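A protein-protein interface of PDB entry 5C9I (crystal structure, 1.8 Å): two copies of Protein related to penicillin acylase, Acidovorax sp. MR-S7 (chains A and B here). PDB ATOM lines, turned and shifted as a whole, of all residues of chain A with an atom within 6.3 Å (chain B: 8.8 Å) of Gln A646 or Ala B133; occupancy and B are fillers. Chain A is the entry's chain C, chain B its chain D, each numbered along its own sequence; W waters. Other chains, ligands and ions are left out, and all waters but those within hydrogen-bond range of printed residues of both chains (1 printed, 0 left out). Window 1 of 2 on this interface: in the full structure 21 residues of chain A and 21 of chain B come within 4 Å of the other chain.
Of chain B, only Ala B133 comes within 4 Å of Gln A646. Ala B133 touches just these residues of chain A: Ala A642 and Gln A646. No residue of chain B comes within 4 Å of Gly A645. Printed residues of chain B within 4 Å of Thr A639: Glu B137 (2.6 Å). Of the printed residues of chain A, Glu B137 touches Thr A639. Of the printed residues of chain B, Ala A642 touches Ala B132 and Ala B133. Of the printed residues of chain A, Ala B132 touches Ala A642 (3.3 Å). Val B140 touches none of the printed residues of chain A. Val B69 touches none of the printed residues of chain A. The nearest residue of chain A that does not touch Ala B133 is Arg A643 (5.4 Å).
No position is printed for both chains. Of the 4 pairs that touch across the chains among the printed residues, none has its exchanged pair printed and touching as well.
Ala A642 touches Ala B132 (CB to O, 3.3 Å). CB of Ala A642 touches O of Ala B133, at 3.6 Å. Gln A646 touches Ala B133.
Water W1 lies within hydrogen-bond range of O of Ala A642 (2.8 Å), N of Gln A646 (3.1 Å), N of Ala B133 (3.4 Å) and O of Ala B132 (3.4 Å).
Of the 12 printed residues of chain A, 3 touch a printed residue of chain B. Of the 22 printed residues of chain B, 3 touch a printed residue of chain A. Hydrophobic or aromatic side chains of chain B within 4 Å of the printed part of chain A: Ala B133. Among the printed residues, 4 pairs touch across the chains.
The guanidinium group (NH1) of Arg A643 lies within hydrogen-bond range of the side-chain amide oxygen (OE1) of Gln A646 (3.5 Å). SG of Cys B45 is disulfide-bonded to SG of Cys B134.
The side-chain carboxylate (OE2) of Glu B137 lies within hydrogen-bond range of the side-chain hydroxyl (OG1) of Thr A639, 2.6 Å away.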
ATOM      1  N   THR A 639       6.722 -12.532  20.950  1.00  0.00           N
ATOM      2  CA  THR A 639       6.041 -11.364  20.341  1.00  0.00           C
ATOM      3  C   THR A 639       4.967 -11.770  19.282  1.00  0.00           C
ATOM      4  O   THR A 639       3.843 -11.231  19.270  1.00  0.00           O
ATOM      5  CB  THR A 639       7.034 -10.306  19.775  1.00  0.00           C
ATOM      6  OG1 THR A 639       7.914  -9.898  20.830  1.00  0.00           O
ATOM      7  CG2 THR A 639       6.238  -9.049  19.302  1.00  0.00           C
ATOM      8  N   ILE A 641       3.261 -14.622  18.990  1.00  0.00           N
ATOM      9  CA  ILE A 641       2.088 -15.234  19.641  1.00  0.00           C
ATOM     10  C   ILE A 641       1.208 -14.081  20.202  1.00  0.00           C
ATOM     11  O   ILE A 641      -0.014 -14.090  20.062  1.00  0.00           O
ATOM     12  CB  ILE A 641       2.595 -16.147  20.800  1.00  0.00           C
ATOM     13  CG1 ILE A 641       3.298 -17.384  20.182  1.00  0.00           C
ATOM     14  CG2 ILE A 641       1.495 -16.501  21.790  1.00  0.00           C
ATOM     15  CD1 ILE A 641       3.991 -18.191  21.299  1.00  0.00           C
ATOM     16  N   ALA A 642       1.835 -13.088  20.824  1.00  0.00           N
ATOM     17  CA  ALA A 642       1.102 -11.949  21.416  1.00  0.00           C
ATOM     18  C   ALA A 642       0.339 -11.129  20.332  1.00  0.00           C
ATOM     19  O   ALA A 642      -0.811 -10.759  20.524  1.00  0.00           O
ATOM     20  CB  ALA A 642       2.016 -11.035  22.284  1.00  0.00           C
ATOM     21  N   ARG A 643       0.991 -10.835  19.236  1.00  0.00           N
ATOM     22  CA  ARG A 643       0.372 -10.061  18.167  1.00  0.00           C
ATOM     23  C   ARG A 643      -0.819 -10.853  17.570  1.00  0.00           C
ATOM     24  O   ARG A 643      -1.919 -10.267  17.369  1.00  0.00           O
ATOM     25  CB  ARG A 643       1.358  -9.735  17.040  1.00  0.00           C
ATOM     26  CG  ARG A 643       2.540  -8.858  17.427  1.00  0.00           C
ATOM     27  CD  ARG A 643       2.085  -7.509  18.015  1.00  0.00           C
ATOM     28  NE  ARG A 643       1.596  -6.588  16.944  1.00  0.00           N
ATOM     29  CZ  ARG A 643       1.195  -5.314  17.139  1.00  0.00           C
ATOM     30  NH1 ARG A 643       1.199  -4.755  18.363  1.00  0.00           N
ATOM     31  NH2 ARG A 643       0.792  -4.579  16.115  1.00  0.00           N
ATOM     32  N   VAL A 644      -0.631 -12.152  17.274  1.00  0.00           N
ATOM     33  CA  VAL A 644      -1.774 -12.966  16.808  1.00  0.00           C
ATOM     34  C   VAL A 644      -2.919 -12.959  17.867  1.00  0.00           C
ATOM     35  O   VAL A 644      -4.100 -12.776  17.503  1.00  0.00           O
ATOM     36  CB  VAL A 644      -1.361 -14.427  16.480  1.00  0.00           C
ATOM     37  CG1 VAL A 644      -2.626 -15.224  16.073  1.00  0.00           C
ATOM     38  CG2 VAL A 644      -0.350 -14.439  15.281  1.00  0.00           C
ATOM     39  N   GLY A 645      -2.599 -13.114  19.149  1.00  0.00           N
ATOM     40  CA  GLY A 645      -3.661 -13.090  20.213  1.00  0.00           C
ATOM     41  C   GLY A 645      -4.374 -11.754  20.244  1.00  0.00           C
ATOM     42  O   GLY A 645      -5.590 -11.667  20.425  1.00  0.00           O
ATOM     43  N   GLN A 646      -3.607 -10.683  20.087  1.00  0.00           N
ATOM     44  CA  GLN A 646      -4.191  -9.311  20.090  1.00  0.00           C
ATOM     45  C   GLN A 646      -5.113  -9.178  18.898  1.00  0.00           C
ATOM     46  O   GLN A 646      -6.139  -8.506  19.025  1.00  0.00           O
ATOM     47  CB  GLN A 646      -3.075  -8.240  20.036  1.00  0.00           C
ATOM     48  CG  GLN A 646      -3.561  -6.792  20.166  1.00  0.00           C
ATOM     49  CD  GLN A 646      -2.418  -5.787  20.195  1.00  0.00           C
ATOM     50  OE1 GLN A 646      -1.258  -6.153  20.371  1.00  0.00           O
ATOM     51  NE2 GLN A 646      -2.740  -4.512  19.931  1.00  0.00           N
ATOM     52  N   SER A 647      -4.758  -9.720  17.738  1.00  0.00           N
ATOM     53  CA  SER A 647      -5.628  -9.672  16.518  1.00  0.00           C
ATOM     54  C   SER A 647      -6.980 -10.335  16.682  1.00  0.00           C
ATOM     55  O   SER A 647      -7.870 -10.107  15.850  1.00  0.00           O
ATOM     56  CB  SER A 647      -4.991 -10.360  15.286  1.00  0.00           C
ATOM     57  OG  SER A 647      -5.027 -11.788  15.420  1.00  0.00           O
ATOM     58  N   GLY A 648      -7.115 -11.190  17.694  1.00  0.00           N
ATOM     59  CA  GLY A 648      -8.317 -11.970  17.863  1.00  0.00           C
ATOM     60  C   GLY A 648      -8.404 -13.239  17.039  1.00  0.00           C
ATOM     61  O   GLY A 648      -9.338 -13.978  17.208  1.00  0.00           O
ATOM     62  N   TYR A 649      -7.504 -13.456  16.074  1.00  0.00           N
ATOM     63  CA  TYR A 649      -7.337 -14.750  15.406  1.00  0.00           C
ATOM     64  C   TYR A 649      -6.697 -15.839  16.277  1.00  0.00           C
ATOM     65  O   TYR A 649      -5.840 -15.541  17.107  1.00  0.00           O
ATOM     66  CB  TYR A 649      -6.458 -14.583  14.135  1.00  0.00           C
ATOM     67  CG  TYR A 649      -7.150 -13.809  13.025  1.00  0.00           C
ATOM     68  CD1 TYR A 649      -8.142 -14.399  12.258  1.00  0.00           C
ATOM     69  CD2 TYR A 649      -6.853 -12.451  12.780  1.00  0.00           C
ATOM     70  CE1 TYR A 649      -8.810 -13.715  11.234  1.00  0.00           C
ATOM     71  CE2 TYR A 649      -7.511 -11.760  11.736  1.00  0.00           C
ATOM     72  CZ  TYR A 649      -8.496 -12.413  10.969  1.00  0.00           C
ATOM     73  OH  TYR A 649      -9.144 -11.780   9.890  1.00  0.00           O
ATOM     74  N   ILE A 689      -1.811  -7.060  11.396  1.00  0.00           N
ATOM     75  CA  ILE A 689      -2.737  -8.153  11.768  1.00  0.00           C
ATOM     76  C   ILE A 689      -3.715  -7.742  12.918  1.00  0.00           C
ATOM     77  O   ILE A 689      -4.850  -8.211  12.937  1.00  0.00           O
ATOM     78  CB  ILE A 689      -1.993  -9.484  12.134  1.00  0.00           C
ATOM     79  CG1 ILE A 689      -2.961 -10.674  12.010  1.00  0.00           C
ATOM     80  CG2 ILE A 689      -1.288  -9.350  13.518  1.00  0.00           C
ATOM     81  CD1 ILE A 689      -2.391 -12.042  12.362  1.00  0.00           C
ATOM     82  N   THR A 690      -3.272  -6.876  13.817  1.00  0.00           N
ATOM     83  CA  THR A 690      -4.098  -6.487  14.968  1.00  0.00           C
ATOM     84  C   THR A 690      -5.202  -5.510  14.568  1.00  0.00           C
ATOM     85  O   THR A 690      -6.014  -5.124  15.412  1.00  0.00           O
ATOM     86  CB  THR A 690      -3.268  -5.842  16.097  1.00  0.00           C
ATOM     87  OG1 THR A 690      -2.664  -4.643  15.620  1.00  0.00           O
ATOM     88  CG2 THR A 690      -2.160  -6.787  16.559  1.00  0.00           C
ATOM     89  N   LEU B  44      -2.207  -2.852  32.237  1.00  0.00           N
ATOM     90  CA  LEU B  44      -0.756  -2.991  32.215  1.00  0.00           C
ATOM     91  C   LEU B  44      -0.135  -2.532  30.840  1.00  0.00           C
ATOM     92  O   LEU B  44       0.879  -1.846  30.827  1.00  0.00           O
ATOM     93  CB  LEU B  44      -0.381  -4.478  32.438  1.00  0.00           C
ATOM     94  CG  LEU B  44       1.104  -4.814  32.481  1.00  0.00           C
ATOM     95  CD1 LEU B  44       1.881  -3.940  33.485  1.00  0.00           C
ATOM     96  CD2 LEU B  44       1.228  -6.338  32.735  1.00  0.00           C
ATOM     97  N   CYS B  45      -0.663  -2.981  29.720  1.00  0.00           N
ATOM     98  CA  CYS B  45      -0.006  -2.753  28.441  1.00  0.00           C
ATOM     99  C   CYS B  45       0.066  -1.273  28.092  1.00  0.00           C
ATOM    100  O   CYS B  45       1.123  -0.814  27.738  1.00  0.00           O
ATOM    101  CB  CYS B  45      -0.609  -3.571  27.291  1.00  0.00           C
ATOM    102  SG  CYS B  45      -0.466  -5.365  27.574  1.00  0.00           S
ATOM    103  N   THR B  46      -1.022  -0.523  28.338  1.00  0.00           N
ATOM    104  CA  THR B  46      -1.003   0.933  28.142  1.00  0.00           C
ATOM    105  C   THR B  46      -0.020   1.552  29.101  1.00  0.00           C
ATOM    106  O   THR B  46       0.805   2.387  28.706  1.00  0.00           O
ATOM    107  CB  THR B  46      -2.419   1.514  28.379  1.00  0.00           C
ATOM    108  OG1 THR B  46      -3.249   0.975  27.345  1.00  0.00           O
ATOM    109  CG2 THR B  46      -2.431   3.049  28.286  1.00  0.00           C
ATOM    110  N   VAL B  69       2.800   4.905  20.218  1.00  0.00           N
ATOM    111  CA  VAL B  69       1.682   3.971  19.928  1.00  0.00           C
ATOM    112  C   VAL B  69       0.308   4.655  20.167  1.00  0.00           C
ATOM    113  O   VAL B  69      -0.658   4.482  19.403  1.00  0.00           O
ATOM    114  CB  VAL B  69       1.787   2.686  20.805  1.00  0.00           C
ATOM    115  CG1 VAL B  69       0.482   1.879  20.797  1.00  0.00           C
ATOM    116  CG2 VAL B  69       2.983   1.828  20.302  1.00  0.00           C
ATOM    117  N   TYR B  70       0.236   5.395  21.278  1.00  0.00           N
ATOM    118  CA  TYR B  70      -1.029   5.991  21.705  1.00  0.00           C
ATOM    119  C   TYR B  70      -1.023   7.498  21.580  1.00  0.00           C
ATOM    120  O   TYR B  70      -0.007   8.157  21.928  1.00  0.00           O
ATOM    121  CB  TYR B  70      -1.288   5.671  23.163  1.00  0.00           C
ATOM    122  CG  TYR B  70      -1.400   4.184  23.455  1.00  0.00           C
ATOM    123  CD1 TYR B  70      -2.563   3.434  23.122  1.00  0.00           C
ATOM    124  CD2 TYR B  70      -0.313   3.517  24.026  1.00  0.00           C
ATOM    125  CE1 TYR B  70      -2.630   2.067  23.461  1.00  0.00           C
ATOM    126  CE2 TYR B  70      -0.352   2.153  24.322  1.00  0.00           C
ATOM    127  CZ  TYR B  70      -1.512   1.434  24.043  1.00  0.00           C
ATOM    128  OH  TYR B  70      -1.486   0.074  24.360  1.00  0.00           O
ATOM    129  N   GLY B 128      -0.558 -16.591  33.694  1.00  0.00           N
ATOM    130  CA  GLY B 128      -1.866 -15.982  33.464  1.00  0.00           C
ATOM    131  C   GLY B 128      -2.055 -15.689  31.993  1.00  0.00           C
ATOM    132  O   GLY B 128      -1.100 -15.762  31.180  1.00  0.00           O
ATOM    133  N   SER B 129      -3.287 -15.371  31.628  1.00  0.00           N
ATOM    134  CA  SER B 129      -3.498 -14.956  30.231  1.00  0.00           C
ATOM    135  C   SER B 129      -4.004 -13.519  30.156  1.00  0.00           C
ATOM    136  O   SER B 129      -4.390 -13.050  29.088  1.00  0.00           O
ATOM    137  CB  SER B 129      -4.420 -15.950  29.497  1.00  0.00           C
ATOM    138  OG  SER B 129      -5.618 -15.998  30.256  1.00  0.00           O
ATOM    139  N   ALA B 130      -3.956 -12.804  31.281  1.00  0.00           N
ATOM    140  CA  ALA B 130      -4.279 -11.386  31.242  1.00  0.00           C
ATOM    141  C   ALA B 130      -3.137 -10.644  30.584  1.00  0.00           C
ATOM    142  O   ALA B 130      -1.943 -10.988  30.812  1.00  0.00           O
ATOM    143  CB  ALA B 130      -4.508 -10.857  32.700  1.00  0.00           C
ATOM    144  N   HIS B 131      -3.473  -9.649  29.748  1.00  0.00           N
ATOM    145  CA  HIS B 131      -2.443  -8.781  29.113  1.00  0.00           C
ATOM    146  C   HIS B 131      -1.528  -9.595  28.266  1.00  0.00           C
ATOM    147  O   HIS B 131      -0.331  -9.324  28.205  1.00  0.00           O
ATOM    148  CB  HIS B 131      -1.610  -8.059  30.170  1.00  0.00           C
ATOM    149  CG  HIS B 131      -2.468  -7.394  31.192  1.00  0.00           C
ATOM    150  ND1 HIS B 131      -3.252  -6.342  30.891  1.00  0.00           N
ATOM    151  CD2 HIS B 131      -2.703  -7.716  32.530  1.00  0.00           C
ATOM    152  CE1 HIS B 131      -3.942  -5.958  31.982  1.00  0.00           C
ATOM    153  NE2 HIS B 131      -3.626  -6.814  32.994  1.00  0.00           N
ATOM    154  N   ALA B 132      -2.116 -10.575  27.616  1.00  0.00           N
ATOM    155  CA  ALA B 132      -1.417 -11.421  26.656  1.00  0.00           C
ATOM    156  C   ALA B 132      -0.694 -10.584  25.616  1.00  0.00           C
ATOM    157  O   ALA B 132       0.289 -11.028  25.050  1.00  0.00           O
ATOM    158  CB  ALA B 132      -2.381 -12.375  25.995  1.00  0.00           C
ATOM    159  N   ALA B 133      -1.242  -9.399  25.302  1.00  0.00           N
ATOM    160  CA  ALA B 133      -0.673  -8.583  24.226  1.00  0.00           C
ATOM    161  C   ALA B 133       0.766  -8.112  24.562  1.00  0.00           C
ATOM    162  O   ALA B 133       1.532  -7.772  23.637  1.00  0.00           O
ATOM    163  CB  ALA B 133      -1.581  -7.378  23.896  1.00  0.00           C
ATOM    164  N   CYS B 134       1.147  -8.102  25.843  1.00  0.00           N
ATOM    165  CA  CYS B 134       2.458  -7.519  26.169  1.00  0.00           C
ATOM    166  C   CYS B 134       3.198  -8.137  27.361  1.00  0.00           C
ATOM    167  O   CYS B 134       4.349  -7.738  27.635  1.00  0.00           O
ATOM    168  CB  CYS B 134       2.303  -6.004  26.462  1.00  0.00           C
ATOM    169  SG  CYS B 134       1.526  -5.637  28.077  1.00  0.00           S
ATOM    170  N   ARG B 135       2.540  -9.053  28.076  1.00  0.00           N
ATOM    171  CA  ARG B 135       3.109  -9.559  29.361  1.00  0.00           C
ATOM    172  C   ARG B 135       4.543 -10.146  29.219  1.00  0.00           C
ATOM    173  O   ARG B 135       5.297 -10.117  30.208  1.00  0.00           O
ATOM    174  CB  ARG B 135       2.148 -10.515  30.076  1.00  0.00           C
ATOM    175  CG  ARG B 135       1.774 -11.749  29.226  1.00  0.00           C
ATOM    176  CD  ARG B 135       0.977 -12.804  30.037  1.00  0.00           C
ATOM    177  NE  ARG B 135       1.836 -13.360  31.101  1.00  0.00           N
ATOM    178  CZ  ARG B 135       2.695 -14.365  30.889  1.00  0.00           C
ATOM    179  NH1 ARG B 135       2.753 -14.957  29.660  1.00  0.00           N
ATOM    180  NH2 ARG B 135       3.508 -14.793  31.874  1.00  0.00           N
ATOM    181  N   SER B 136       4.953 -10.599  28.020  1.00  0.00           N
ATOM    182  CA  SER B 136       6.244 -11.238  27.895  1.00  0.00           C
ATOM    183  C   SER B 136       7.257 -10.296  27.231  1.00  0.00           C
ATOM    184  O   SER B 136       8.399 -10.701  26.950  1.00  0.00           O
ATOM    185  CB  SER B 136       6.132 -12.607  27.183  1.00  0.00           C
ATOM    186  OG  SER B 136       5.598 -12.420  25.875  1.00  0.00           O
ATOM    187  N   GLU B 137       6.893  -9.029  27.007  1.00  0.00           N
ATOM    188  CA  GLU B 137       7.837  -8.076  26.377  1.00  0.00           C
ATOM    189  C   GLU B 137       8.840  -7.504  27.398  1.00  0.00           C
ATOM    190  O   GLU B 137       8.483  -7.431  28.557  1.00  0.00           O
ATOM    191  CB  GLU B 137       7.056  -6.909  25.757  1.00  0.00           C
ATOM    192  CG  GLU B 137       6.167  -7.367  24.598  1.00  0.00           C
ATOM    193  CD  GLU B 137       6.981  -7.907  23.420  1.00  0.00           C
ATOM    194  OE1 GLU B 137       8.200  -7.597  23.247  1.00  0.00           O
ATOM    195  OE2 GLU B 137       6.452  -8.709  22.651  1.00  0.00           O
ATOM    196  N   TRP B 139       9.793  -4.508  27.936  1.00  0.00           N
ATOM    197  CA  TRP B 139       9.348  -3.232  28.470  1.00  0.00           C
ATOM    198  C   TRP B 139       8.211  -3.348  29.451  1.00  0.00           C
ATOM    199  O   TRP B 139       7.814  -2.350  30.095  1.00  0.00           O
ATOM    200  CB  TRP B 139       8.983  -2.319  27.326  1.00  0.00           C
ATOM    201  CG  TRP B 139       8.115  -2.904  26.262  1.00  0.00           C
ATOM    202  CD1 TRP B 139       8.541  -3.496  25.072  1.00  0.00           C
ATOM    203  CD2 TRP B 139       6.644  -2.897  26.209  1.00  0.00           C
ATOM    204  NE1 TRP B 139       7.452  -3.895  24.335  1.00  0.00           N
ATOM    205  CE2 TRP B 139       6.284  -3.507  24.933  1.00  0.00           C
ATOM    206  CE3 TRP B 139       5.639  -2.364  27.011  1.00  0.00           C
ATOM    207  CZ2 TRP B 139       4.964  -3.667  24.537  1.00  0.00           C
ATOM    208  CZ3 TRP B 139       4.300  -2.523  26.589  1.00  0.00           C
ATOM    209  CH2 TRP B 139       3.983  -3.171  25.373  1.00  0.00           C
ATOM    210  N   VAL B 140       7.707  -4.560  29.652  1.00  0.00           N
ATOM    211  CA  VAL B 140       6.920  -4.789  30.871  1.00  0.00           C
ATOM    212  C   VAL B 140       7.943  -5.040  31.989  1.00  0.00           C
ATOM    213  O   VAL B 140       8.594  -6.079  32.020  1.00  0.00           O
ATOM    214  CB  VAL B 140       5.881  -5.925  30.693  1.00  0.00           C
ATOM    215  CG1 VAL B 140       5.207  -6.198  32.028  1.00  0.00           C
ATOM    216  CG2 VAL B 140       4.828  -5.417  29.703  1.00  0.00           C
ATOM    217  N   LYS B 225      -8.044   5.734  24.442  1.00  0.00           N
ATOM    218  CA  LYS B 225      -6.903   4.819  24.625  1.00  0.00           C
ATOM    219  C   LYS B 225      -5.692   5.674  25.048  1.00  0.00           C
ATOM    220  O   LYS B 225      -5.721   6.937  24.892  1.00  0.00           O
ATOM    221  CB  LYS B 225      -6.539   4.067  23.337  1.00  0.00           C
ATOM    222  CG  LYS B 225      -7.652   3.141  22.766  1.00  0.00           C
ATOM    223  CD  LYS B 225      -7.127   2.304  21.634  1.00  0.00           C
ATOM    224  CE  LYS B 225      -8.171   1.249  21.258  1.00  0.00           C
ATOM    225  NZ  LYS B 225      -7.738   0.601  19.978  1.00  0.00           N
ATOM    226  N   ASP B 729      -8.000  -2.012  29.344  1.00  0.00           N
ATOM    227  CA  ASP B 729      -7.550  -2.033  27.906  1.00  0.00           C
ATOM    228  C   ASP B 729      -7.312  -3.462  27.356  1.00  0.00           C
ATOM    229  O   ASP B 729      -6.986  -3.646  26.169  1.00  0.00           O
ATOM    230  CB  ASP B 729      -6.280  -1.172  27.695  1.00  0.00           C
ATOM    231  CG  ASP B 729      -5.027  -1.787  28.316  1.00  0.00           C
ATOM    232  OD1 ASP B 729      -5.158  -2.701  29.128  1.00  0.00           O
ATOM    233  OD2 ASP B 729      -3.886  -1.416  27.950  1.00  0.00           O
ATOM    234  N   ASP B 730      -7.567  -4.460  28.170  1.00  0.00           N
ATOM    235  CA  ASP B 730      -7.243  -5.877  27.796  1.00  0.00           C
ATOM    236  C   ASP B 730      -8.495  -6.555  27.182  1.00  0.00           C
ATOM    237  O   ASP B 730      -9.500  -6.740  27.886  1.00  0.00           O
ATOM    238  CB  ASP B 730      -6.808  -6.592  29.091  1.00  0.00           C
ATOM    239  CG  ASP B 730      -6.387  -8.058  28.896  1.00  0.00           C
ATOM    240  OD1 ASP B 730      -6.414  -8.586  27.738  1.00  0.00           O
ATOM    241  OD2 ASP B 730      -6.002  -8.697  29.912  1.00  0.00           O
ATOM    242  N   PRO B 731      -8.450  -6.928  25.872  1.00  0.00           N
ATOM    243  CA  PRO B 731      -9.631  -7.600  25.269  1.00  0.00           C
ATOM    244  C   PRO B 731     -10.117  -8.825  26.065  1.00  0.00           C
ATOM    245  O   PRO B 731     -11.276  -9.176  25.934  1.00  0.00           O
ATOM    246  CB  PRO B 731      -9.084  -8.129  23.922  1.00  0.00           C
ATOM    247  CG  PRO B 731      -7.921  -7.242  23.613  1.00  0.00           C
ATOM    248  CD  PRO B 731      -7.274  -7.009  24.968  1.00  0.00           C
ATOM    249  N   ALA B 732      -9.268  -9.451  26.893  1.00  0.00           N
ATOM    250  CA  ALA B 732      -9.684 -10.655  27.615  1.00  0.00           C
ATOM    251  C   ALA B 732     -10.457 -10.290  28.885  1.00  0.00           C
ATOM    252  O   ALA B 732     -10.981 -11.173  29.535  1.00  0.00           O
ATOM    253  CB  ALA B 732      -8.471 -11.538  27.987  1.00  0.00           C
HETATM  254  O   HOH W   1      -2.290 -11.484  22.832  1.00  0.00           O
